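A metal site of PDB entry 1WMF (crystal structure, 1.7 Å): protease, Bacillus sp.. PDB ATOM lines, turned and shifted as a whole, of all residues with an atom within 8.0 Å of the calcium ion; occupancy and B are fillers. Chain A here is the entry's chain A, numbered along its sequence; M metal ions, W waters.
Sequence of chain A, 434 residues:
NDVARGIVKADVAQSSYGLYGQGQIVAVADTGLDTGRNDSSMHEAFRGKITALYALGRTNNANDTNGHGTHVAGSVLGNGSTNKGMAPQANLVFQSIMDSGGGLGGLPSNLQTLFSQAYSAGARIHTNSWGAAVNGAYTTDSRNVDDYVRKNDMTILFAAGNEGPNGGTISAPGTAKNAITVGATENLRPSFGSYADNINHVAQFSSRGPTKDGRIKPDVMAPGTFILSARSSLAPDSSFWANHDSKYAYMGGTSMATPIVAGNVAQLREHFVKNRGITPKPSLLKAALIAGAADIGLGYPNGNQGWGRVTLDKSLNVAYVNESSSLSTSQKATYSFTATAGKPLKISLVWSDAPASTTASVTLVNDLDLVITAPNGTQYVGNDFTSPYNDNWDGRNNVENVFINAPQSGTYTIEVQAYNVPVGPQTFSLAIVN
The side-chain carboxylate (OE1) of Glu 400 sits at hydrogen-bond distance from the backbone NH (N) of Leu 370 (2.8 Å).
The backbone NH (N) of Glu 400 lies within hydrogen-bond range of the backbone carbonyl oxygen (O) of Leu 349.
The backbone carbonyl oxygen of Asp 369 lies within hydrogen-bond range of the backbone NH of Gln 417, 2.8 Å away.
The backbone carbonyl oxygen of Asp 367 lies within hydrogen-bond range of the backbone NH of Tyr 419, at 2.8 Å.
O of Asn 420 is in hydrogen-bond range of N of Asp 367, at 2.8 Å.
The side-chain amide nitrogen (ND2) of Asn 397 sits at hydrogen-bond distance from the side-chain carboxylate (OD2) of Asp 394 (2.8 Å).
N of Arg 396 lies within hydrogen-bond range of OD1 of Asp 394, 2.8 Å away.
The side-chain carboxylate (OD2) of Asp 394 sits at hydrogen-bond distance from the side-chain amide nitrogen (ND2) of Asn 383 (2.9 Å).
Of the 23 residues printed, 5 come within 4 Å of the calcium ion.
Along chain A the residues within 4 Å of the calcium ion span positions 367 to 400.
The calcium ion is bound by the side-chain carboxylate of Glu 400 (2.2 Å), the side-chain carboxylate of Asp 369 (2.3 Å), the side-chain carboxylate of Asp 367 (2.3 Å), the backbone carbonyl oxygen of Asp 394 (2.3 Å), the backbone carbonyl oxygen of Leu 368 (2.4 Å) and water W1 (2.4 Å).
Water W1 lies within hydrogen-bond range of the side-chain carboxylate (OD1) of Asp 394 and the backbone carbonyl oxygen (O) of Asn 397.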
ATOM      1  N   LEU A 349      -0.608 -19.652  17.810  1.00  0.00           N
ATOM      2  CA  LEU A 349      -1.531 -19.745  18.935  1.00  0.00           C
ATOM      3  C   LEU A 349      -1.538 -21.202  19.430  1.00  0.00           C
ATOM      4  O   LEU A 349      -1.835 -22.104  18.633  1.00  0.00           O
ATOM      5  CB  LEU A 349      -2.931 -19.337  18.486  1.00  0.00           C
ATOM      6  CG  LEU A 349      -4.040 -19.501  19.523  1.00  0.00           C
ATOM      7  CD1 LEU A 349      -3.796 -18.603  20.724  1.00  0.00           C
ATOM      8  CD2 LEU A 349      -5.380 -19.188  18.858  1.00  0.00           C
ATOM      9  N   TRP A 351      -2.742 -23.697  22.895  1.00  0.00           N
ATOM     10  CA  TRP A 351      -3.343 -23.719  24.233  1.00  0.00           C
ATOM     11  C   TRP A 351      -3.223 -25.129  24.846  1.00  0.00           C
ATOM     12  O   TRP A 351      -3.196 -26.112  24.108  1.00  0.00           O
ATOM     13  CB  TRP A 351      -4.793 -23.275  24.295  1.00  0.00           C
ATOM     14  CG  TRP A 351      -5.838 -23.908  23.437  1.00  0.00           C
ATOM     15  CD1 TRP A 351      -6.790 -24.797  23.847  1.00  0.00           C
ATOM     16  CD2 TRP A 351      -6.050 -23.706  22.035  1.00  0.00           C
ATOM     17  NE1 TRP A 351      -7.602 -25.165  22.776  1.00  0.00           N
ATOM     18  CE2 TRP A 351      -7.148 -24.507  21.666  1.00  0.00           C
ATOM     19  CE3 TRP A 351      -5.422 -22.927  21.063  1.00  0.00           C
ATOM     20  CZ2 TRP A 351      -7.636 -24.550  20.361  1.00  0.00           C
ATOM     21  CZ3 TRP A 351      -5.888 -22.965  19.768  1.00  0.00           C
ATOM     22  CH2 TRP A 351      -6.983 -23.778  19.436  1.00  0.00           C
ATOM     23  N   LEU A 364     -10.285 -32.453  20.552  1.00  0.00           N
ATOM     24  CA  LEU A 364     -10.325 -31.045  20.974  1.00  0.00           C
ATOM     25  C   LEU A 364     -11.564 -30.800  21.817  1.00  0.00           C
ATOM     26  O   LEU A 364     -12.681 -31.170  21.418  1.00  0.00           O
ATOM     27  CB  LEU A 364     -10.312 -30.123  19.760  1.00  0.00           C
ATOM     28  CG  LEU A 364     -10.101 -28.631  20.037  1.00  0.00           C
ATOM     29  CD1 LEU A 364      -8.669 -28.391  20.521  1.00  0.00           C
ATOM     30  CD2 LEU A 364     -10.410 -27.805  18.791  1.00  0.00           C
ATOM     31  N   ASN A 366     -11.854 -27.465  23.965  1.00  0.00           N
ATOM     32  CA  ASN A 366     -12.082 -26.037  23.801  1.00  0.00           C
ATOM     33  C   ASN A 366     -11.491 -25.545  22.477  1.00  0.00           C
ATOM     34  O   ASN A 366     -10.309 -25.789  22.188  1.00  0.00           O
ATOM     35  CB  ASN A 366     -11.476 -25.221  24.951  1.00  0.00           C
ATOM     36  CG  ASN A 366     -12.098 -25.587  26.287  1.00  0.00           C
ATOM     37  OD1 ASN A 366     -13.309 -25.796  26.381  1.00  0.00           O
ATOM     38  ND2 ASN A 366     -11.217 -25.635  27.292  1.00  0.00           N
ATOM     39  N   ASP A 367     -12.309 -24.856  21.691  1.00  0.00           N
ATOM     40  CA  ASP A 367     -11.884 -24.422  20.365  1.00  0.00           C
ATOM     41  C   ASP A 367     -11.742 -22.914  20.306  1.00  0.00           C
ATOM     42  O   ASP A 367     -12.710 -22.155  20.358  1.00  0.00           O
ATOM     43  CB  ASP A 367     -12.891 -24.934  19.341  1.00  0.00           C
ATOM     44  CG  ASP A 367     -12.625 -24.575  17.900  1.00  0.00           C
ATOM     45  OD1 ASP A 367     -11.542 -24.066  17.588  1.00  0.00           O
ATOM     46  OD2 ASP A 367     -13.525 -24.802  17.041  1.00  0.00           O
ATOM     47  N   LEU A 368     -10.479 -22.499  20.209  1.00  0.00           N
ATOM     48  CA  LEU A 368     -10.118 -21.134  19.935  1.00  0.00           C
ATOM     49  C   LEU A 368      -9.739 -20.992  18.446  1.00  0.00           C
ATOM     50  O   LEU A 368      -9.197 -21.934  17.860  1.00  0.00           O
ATOM     51  CB  LEU A 368      -8.942 -20.657  20.784  1.00  0.00           C
ATOM     52  CG  LEU A 368      -8.996 -20.960  22.284  1.00  0.00           C
ATOM     53  CD1 LEU A 368      -7.688 -20.570  22.934  1.00  0.00           C
ATOM     54  CD2 LEU A 368     -10.170 -20.225  22.919  1.00  0.00           C
ATOM     55  N   ASP A 369     -10.042 -19.836  17.864  1.00  0.00           N
ATOM     56  CA  ASP A 369      -9.659 -19.533  16.500  1.00  0.00           C
ATOM     57  C   ASP A 369      -8.746 -18.312  16.453  1.00  0.00           C
ATOM     58  O   ASP A 369      -9.023 -17.317  17.125  1.00  0.00           O
ATOM     59  CB  ASP A 369     -10.864 -19.217  15.612  1.00  0.00           C
ATOM     60  CG  ASP A 369     -11.760 -20.428  15.450  1.00  0.00           C
ATOM     61  OD1 ASP A 369     -11.247 -21.557  15.577  1.00  0.00           O
ATOM     62  OD2 ASP A 369     -12.976 -20.266  15.231  1.00  0.00           O
ATOM     63  N   LEU A 370      -7.707 -18.412  15.644  1.00  0.00           N
ATOM     64  CA  LEU A 370      -6.834 -17.279  15.383  1.00  0.00           C
ATOM     65  C   LEU A 370      -7.307 -16.513  14.145  1.00  0.00           C
ATOM     66  O   LEU A 370      -7.515 -17.112  13.088  1.00  0.00           O
ATOM     67  CB  LEU A 370      -5.387 -17.781  15.239  1.00  0.00           C
ATOM     68  CG  LEU A 370      -4.322 -16.725  14.934  1.00  0.00           C
ATOM     69  CD1 LEU A 370      -4.190 -15.753  16.096  1.00  0.00           C
ATOM     70  CD2 LEU A 370      -2.987 -17.393  14.611  1.00  0.00           C
ATOM     71  N   VAL A 381      -7.063 -16.853   8.625  1.00  0.00           N
ATOM     72  CA  VAL A 381      -7.615 -17.752   9.625  1.00  0.00           C
ATOM     73  C   VAL A 381      -6.563 -18.786   9.993  1.00  0.00           C
ATOM     74  O   VAL A 381      -5.868 -19.258   9.099  1.00  0.00           O
ATOM     75  CB  VAL A 381      -8.891 -18.371   9.025  1.00  0.00           C
ATOM     76  CG1 VAL A 381      -9.322 -19.618   9.755  1.00  0.00           C
ATOM     77  CG2 VAL A 381      -9.978 -17.299   9.021  1.00  0.00           C
ATOM     78  N   GLY A 382      -6.411 -19.105  11.279  1.00  0.00           N
ATOM     79  CA  GLY A 382      -5.389 -20.060  11.706  1.00  0.00           C
ATOM     80  C   GLY A 382      -5.448 -21.349  10.899  1.00  0.00           C
ATOM     81  O   GLY A 382      -6.557 -21.864  10.728  1.00  0.00           O
ATOM     82  N   ASN A 383      -4.285 -21.769  10.440  1.00  0.00           N
ATOM     83  CA  ASN A 383      -3.989 -22.976   9.699  1.00  0.00           C
ATOM     84  C   ASN A 383      -4.628 -23.031   8.310  1.00  0.00           C
ATOM     85  O   ASN A 383      -4.673 -24.080   7.673  1.00  0.00           O
ATOM     86  CB  ASN A 383      -4.385 -24.243  10.482  1.00  0.00           C
ATOM     87  CG  ASN A 383      -3.549 -24.379  11.748  1.00  0.00           C
ATOM     88  OD1 ASN A 383      -2.506 -23.734  11.894  1.00  0.00           O
ATOM     89  ND2 ASN A 383      -3.972 -25.220  12.691  1.00  0.00           N
ATOM     90  N   TRP A 393     -11.769 -22.850   8.383  1.00  0.00           N
ATOM     91  CA  TRP A 393     -11.577 -22.778   9.821  1.00  0.00           C
ATOM     92  C   TRP A 393     -11.114 -24.071  10.459  1.00  0.00           C
ATOM     93  O   TRP A 393     -11.444 -25.170  10.003  1.00  0.00           O
ATOM     94  CB  TRP A 393     -12.897 -22.352  10.477  1.00  0.00           C
ATOM     95  CG  TRP A 393     -13.270 -20.982   9.970  1.00  0.00           C
ATOM     96  CD1 TRP A 393     -13.815 -20.662   8.766  1.00  0.00           C
ATOM     97  CD2 TRP A 393     -13.113 -19.775  10.709  1.00  0.00           C
ATOM     98  NE1 TRP A 393     -13.996 -19.297   8.692  1.00  0.00           N
ATOM     99  CE2 TRP A 393     -13.572 -18.740   9.883  1.00  0.00           C
ATOM    100  CE3 TRP A 393     -12.624 -19.470  11.982  1.00  0.00           C
ATOM    101  CZ2 TRP A 393     -13.555 -17.414  10.316  1.00  0.00           C
ATOM    102  CZ3 TRP A 393     -12.598 -18.152  12.401  1.00  0.00           C
ATOM    103  CH2 TRP A 393     -13.069 -17.134  11.570  1.00  0.00           C
ATOM    104  N   ASP A 394     -10.356 -23.953  11.540  1.00  0.00           N
ATOM    105  CA  ASP A 394      -9.838 -25.167  12.177  1.00  0.00           C
ATOM    106  C   ASP A 394     -10.623 -25.448  13.460  1.00  0.00           C
ATOM    107  O   ASP A 394     -10.763 -24.577  14.322  1.00  0.00           O
ATOM    108  CB  ASP A 394      -8.345 -24.964  12.422  1.00  0.00           C
ATOM    109  CG  ASP A 394      -7.641 -26.182  13.018  1.00  0.00           C
ATOM    110  OD1 ASP A 394      -8.139 -26.781  13.982  1.00  0.00           O
ATOM    111  OD2 ASP A 394      -6.553 -26.520  12.487  1.00  0.00           O
ATOM    112  N   GLY A 395     -11.106 -26.674  13.559  1.00  0.00           N
ATOM    113  CA  GLY A 395     -11.904 -27.174  14.669  1.00  0.00           C
ATOM    114  C   GLY A 395     -11.295 -28.441  15.248  1.00  0.00           C
ATOM    115  O   GLY A 395     -11.970 -29.181  15.974  1.00  0.00           O
ATOM    116  N   ARG A 396     -10.014 -28.675  14.932  1.00  0.00           N
ATOM    117  CA  ARG A 396      -9.392 -29.900  15.439  1.00  0.00           C
ATOM    118  C   ARG A 396      -8.125 -29.683  16.249  1.00  0.00           C
ATOM    119  O   ARG A 396      -7.844 -30.430  17.216  1.00  0.00           O
ATOM    120  CB  ARG A 396      -9.091 -30.831  14.247  1.00  0.00           C
ATOM    121  CG  ARG A 396     -10.340 -31.563  13.767  1.00  0.00           C
ATOM    122  CD  ARG A 396     -10.980 -32.414  14.844  1.00  0.00           C
ATOM    123  NE  ARG A 396     -12.044 -33.237  14.264  1.00  0.00           N
ATOM    124  CZ  ARG A 396     -13.279 -32.774  14.164  1.00  0.00           C
ATOM    125  NH1 ARG A 396     -13.559 -31.536  14.597  1.00  0.00           N
ATOM    126  NH2 ARG A 396     -14.231 -33.520  13.639  1.00  0.00           N
ATOM    127  N   ASN A 397      -7.317 -28.683  15.930  1.00  0.00           N
ATOM    128  CA  ASN A 397      -5.996 -28.511  16.530  1.00  0.00           C
ATOM    129  C   ASN A 397      -5.956 -27.524  17.675  1.00  0.00           C
ATOM    130  O   ASN A 397      -6.694 -26.546  17.596  1.00  0.00           O
ATOM    131  CB  ASN A 397      -5.053 -27.990  15.445  1.00  0.00           C
ATOM    132  CG  ASN A 397      -4.773 -29.062  14.410  1.00  0.00           C
ATOM    133  OD1 ASN A 397      -4.180 -30.093  14.740  1.00  0.00           O
ATOM    134  ND2 ASN A 397      -5.185 -28.820  13.178  1.00  0.00           N
ATOM    135  N   ASN A 398      -5.087 -27.768  18.671  1.00  0.00           N
ATOM    136  CA  ASN A 398      -4.916 -26.740  19.710  1.00  0.00           C
ATOM    137  C   ASN A 398      -3.643 -25.920  19.489  1.00  0.00           C
ATOM    138  O   ASN A 398      -3.060 -25.326  20.381  1.00  0.00           O
ATOM    139  CB  ASN A 398      -4.921 -27.358  21.095  1.00  0.00           C
ATOM    140  CG  ASN A 398      -3.971 -28.520  21.263  1.00  0.00           C
ATOM    141  OD1 ASN A 398      -3.931 -29.430  20.421  1.00  0.00           O
ATOM    142  ND2 ASN A 398      -3.216 -28.490  22.359  1.00  0.00           N
ATOM    143  N   VAL A 399      -3.203 -25.912  18.247  1.00  0.00           N
ATOM    144  CA  VAL A 399      -2.184 -25.078  17.654  1.00  0.00           C
ATOM    145  C   VAL A 399      -2.751 -24.448  16.371  1.00  0.00           C
ATOM    146  O   VAL A 399      -3.141 -25.220  15.488  1.00  0.00           O
ATOM    147  CB  VAL A 399      -0.928 -25.880  17.243  1.00  0.00           C
ATOM    148  CG1 VAL A 399       0.111 -24.920  16.678  1.00  0.00           C
ATOM    149  CG2 VAL A 399      -0.355 -26.684  18.406  1.00  0.00           C
ATOM    150  N   GLU A 400      -2.796 -23.120  16.273  1.00  0.00           N
ATOM    151  CA  GLU A 400      -3.264 -22.475  15.049  1.00  0.00           C
ATOM    152  C   GLU A 400      -2.210 -21.476  14.590  1.00  0.00           C
ATOM    153  O   GLU A 400      -1.618 -20.771  15.421  1.00  0.00           O
ATOM    154  CB  GLU A 400      -4.627 -21.809  15.216  1.00  0.00           C
ATOM    155  CG  GLU A 400      -5.802 -22.760  15.217  1.00  0.00           C
ATOM    156  CD  GLU A 400      -7.116 -22.095  14.863  1.00  0.00           C
ATOM    157  OE1 GLU A 400      -7.106 -20.900  14.432  1.00  0.00           O
ATOM    158  OE2 GLU A 400      -8.155 -22.759  15.016  1.00  0.00           O
ATOM    159  N   GLN A 417     -10.160 -15.809  19.152  1.00  0.00           N
ATOM    160  CA  GLN A 417     -11.611 -15.868  19.275  1.00  0.00           C
ATOM    161  C   GLN A 417     -12.062 -17.147  19.944  1.00  0.00           C
ATOM    162  O   GLN A 417     -11.657 -18.254  19.561  1.00  0.00           O
ATOM    163  CB  GLN A 417     -12.233 -15.750  17.866  1.00  0.00           C
ATOM    164  CG  GLN A 417     -11.926 -14.405  17.233  1.00  0.00           C
ATOM    165  CD  GLN A 417     -12.579 -14.237  15.874  1.00  0.00           C
ATOM    166  OE1 GLN A 417     -13.170 -15.197  15.351  1.00  0.00           O
ATOM    167  NE2 GLN A 417     -12.447 -13.059  15.289  1.00  0.00           N
ATOM    168  N   ALA A 418     -12.925 -17.046  20.968  1.00  0.00           N
ATOM    169  CA  ALA A 418     -13.321 -18.323  21.579  1.00  0.00           C
ATOM    170  C   ALA A 418     -14.520 -18.920  20.853  1.00  0.00           C
ATOM    171  O   ALA A 418     -15.661 -18.512  21.073  1.00  0.00           O
ATOM    172  CB  ALA A 418     -13.599 -18.081  23.054  1.00  0.00           C
ATOM    173  N   TYR A 419     -14.329 -19.889  19.955  1.00  0.00           N
ATOM    174  CA  TYR A 419     -15.458 -20.355  19.157  1.00  0.00           C
ATOM    175  C   TYR A 419     -16.403 -21.220  19.965  1.00  0.00           C
ATOM    176  O   TYR A 419     -17.632 -21.111  19.920  1.00  0.00           O
ATOM    177  CB  TYR A 419     -14.941 -21.137  17.929  1.00  0.00           C
ATOM    178  CG  TYR A 419     -16.068 -21.764  17.143  1.00  0.00           C
ATOM    179  CD1 TYR A 419     -16.917 -20.978  16.392  1.00  0.00           C
ATOM    180  CD2 TYR A 419     -16.278 -23.149  17.164  1.00  0.00           C
ATOM    181  CE1 TYR A 419     -17.961 -21.513  15.659  1.00  0.00           C
ATOM    182  CE2 TYR A 419     -17.313 -23.698  16.437  1.00  0.00           C
ATOM    183  CZ  TYR A 419     -18.137 -22.878  15.704  1.00  0.00           C
ATOM    184  OH  TYR A 419     -19.171 -23.429  14.986  1.00  0.00           O
ATOM    185  N   ASN A 420     -15.838 -22.120  20.761  1.00  0.00           N
ATOM    186  CA  ASN A 420     -16.662 -22.998  21.573  1.00  0.00           C
ATOM    187  C   ASN A 420     -15.844 -23.572  22.733  1.00  0.00           C
ATOM    188  O   ASN A 420     -15.003 -24.432  22.502  1.00  0.00           O
ATOM    189  CB  ASN A 420     -17.202 -24.129  20.706  1.00  0.00           C
ATOM    190  CG  ASN A 420     -18.172 -25.000  21.472  1.00  0.00           C
ATOM    191  OD1 ASN A 420     -18.557 -24.693  22.599  1.00  0.00           O
ATOM    192  ND2 ASN A 420     -18.584 -26.098  20.834  1.00  0.00           N
HETATM  193 CA    CA M   1      -9.937 -23.327  16.106  1.00  0.00          CA
HETATM  194  O   HOH W   1      -8.960 -25.524  16.247  1.00  0.00           O
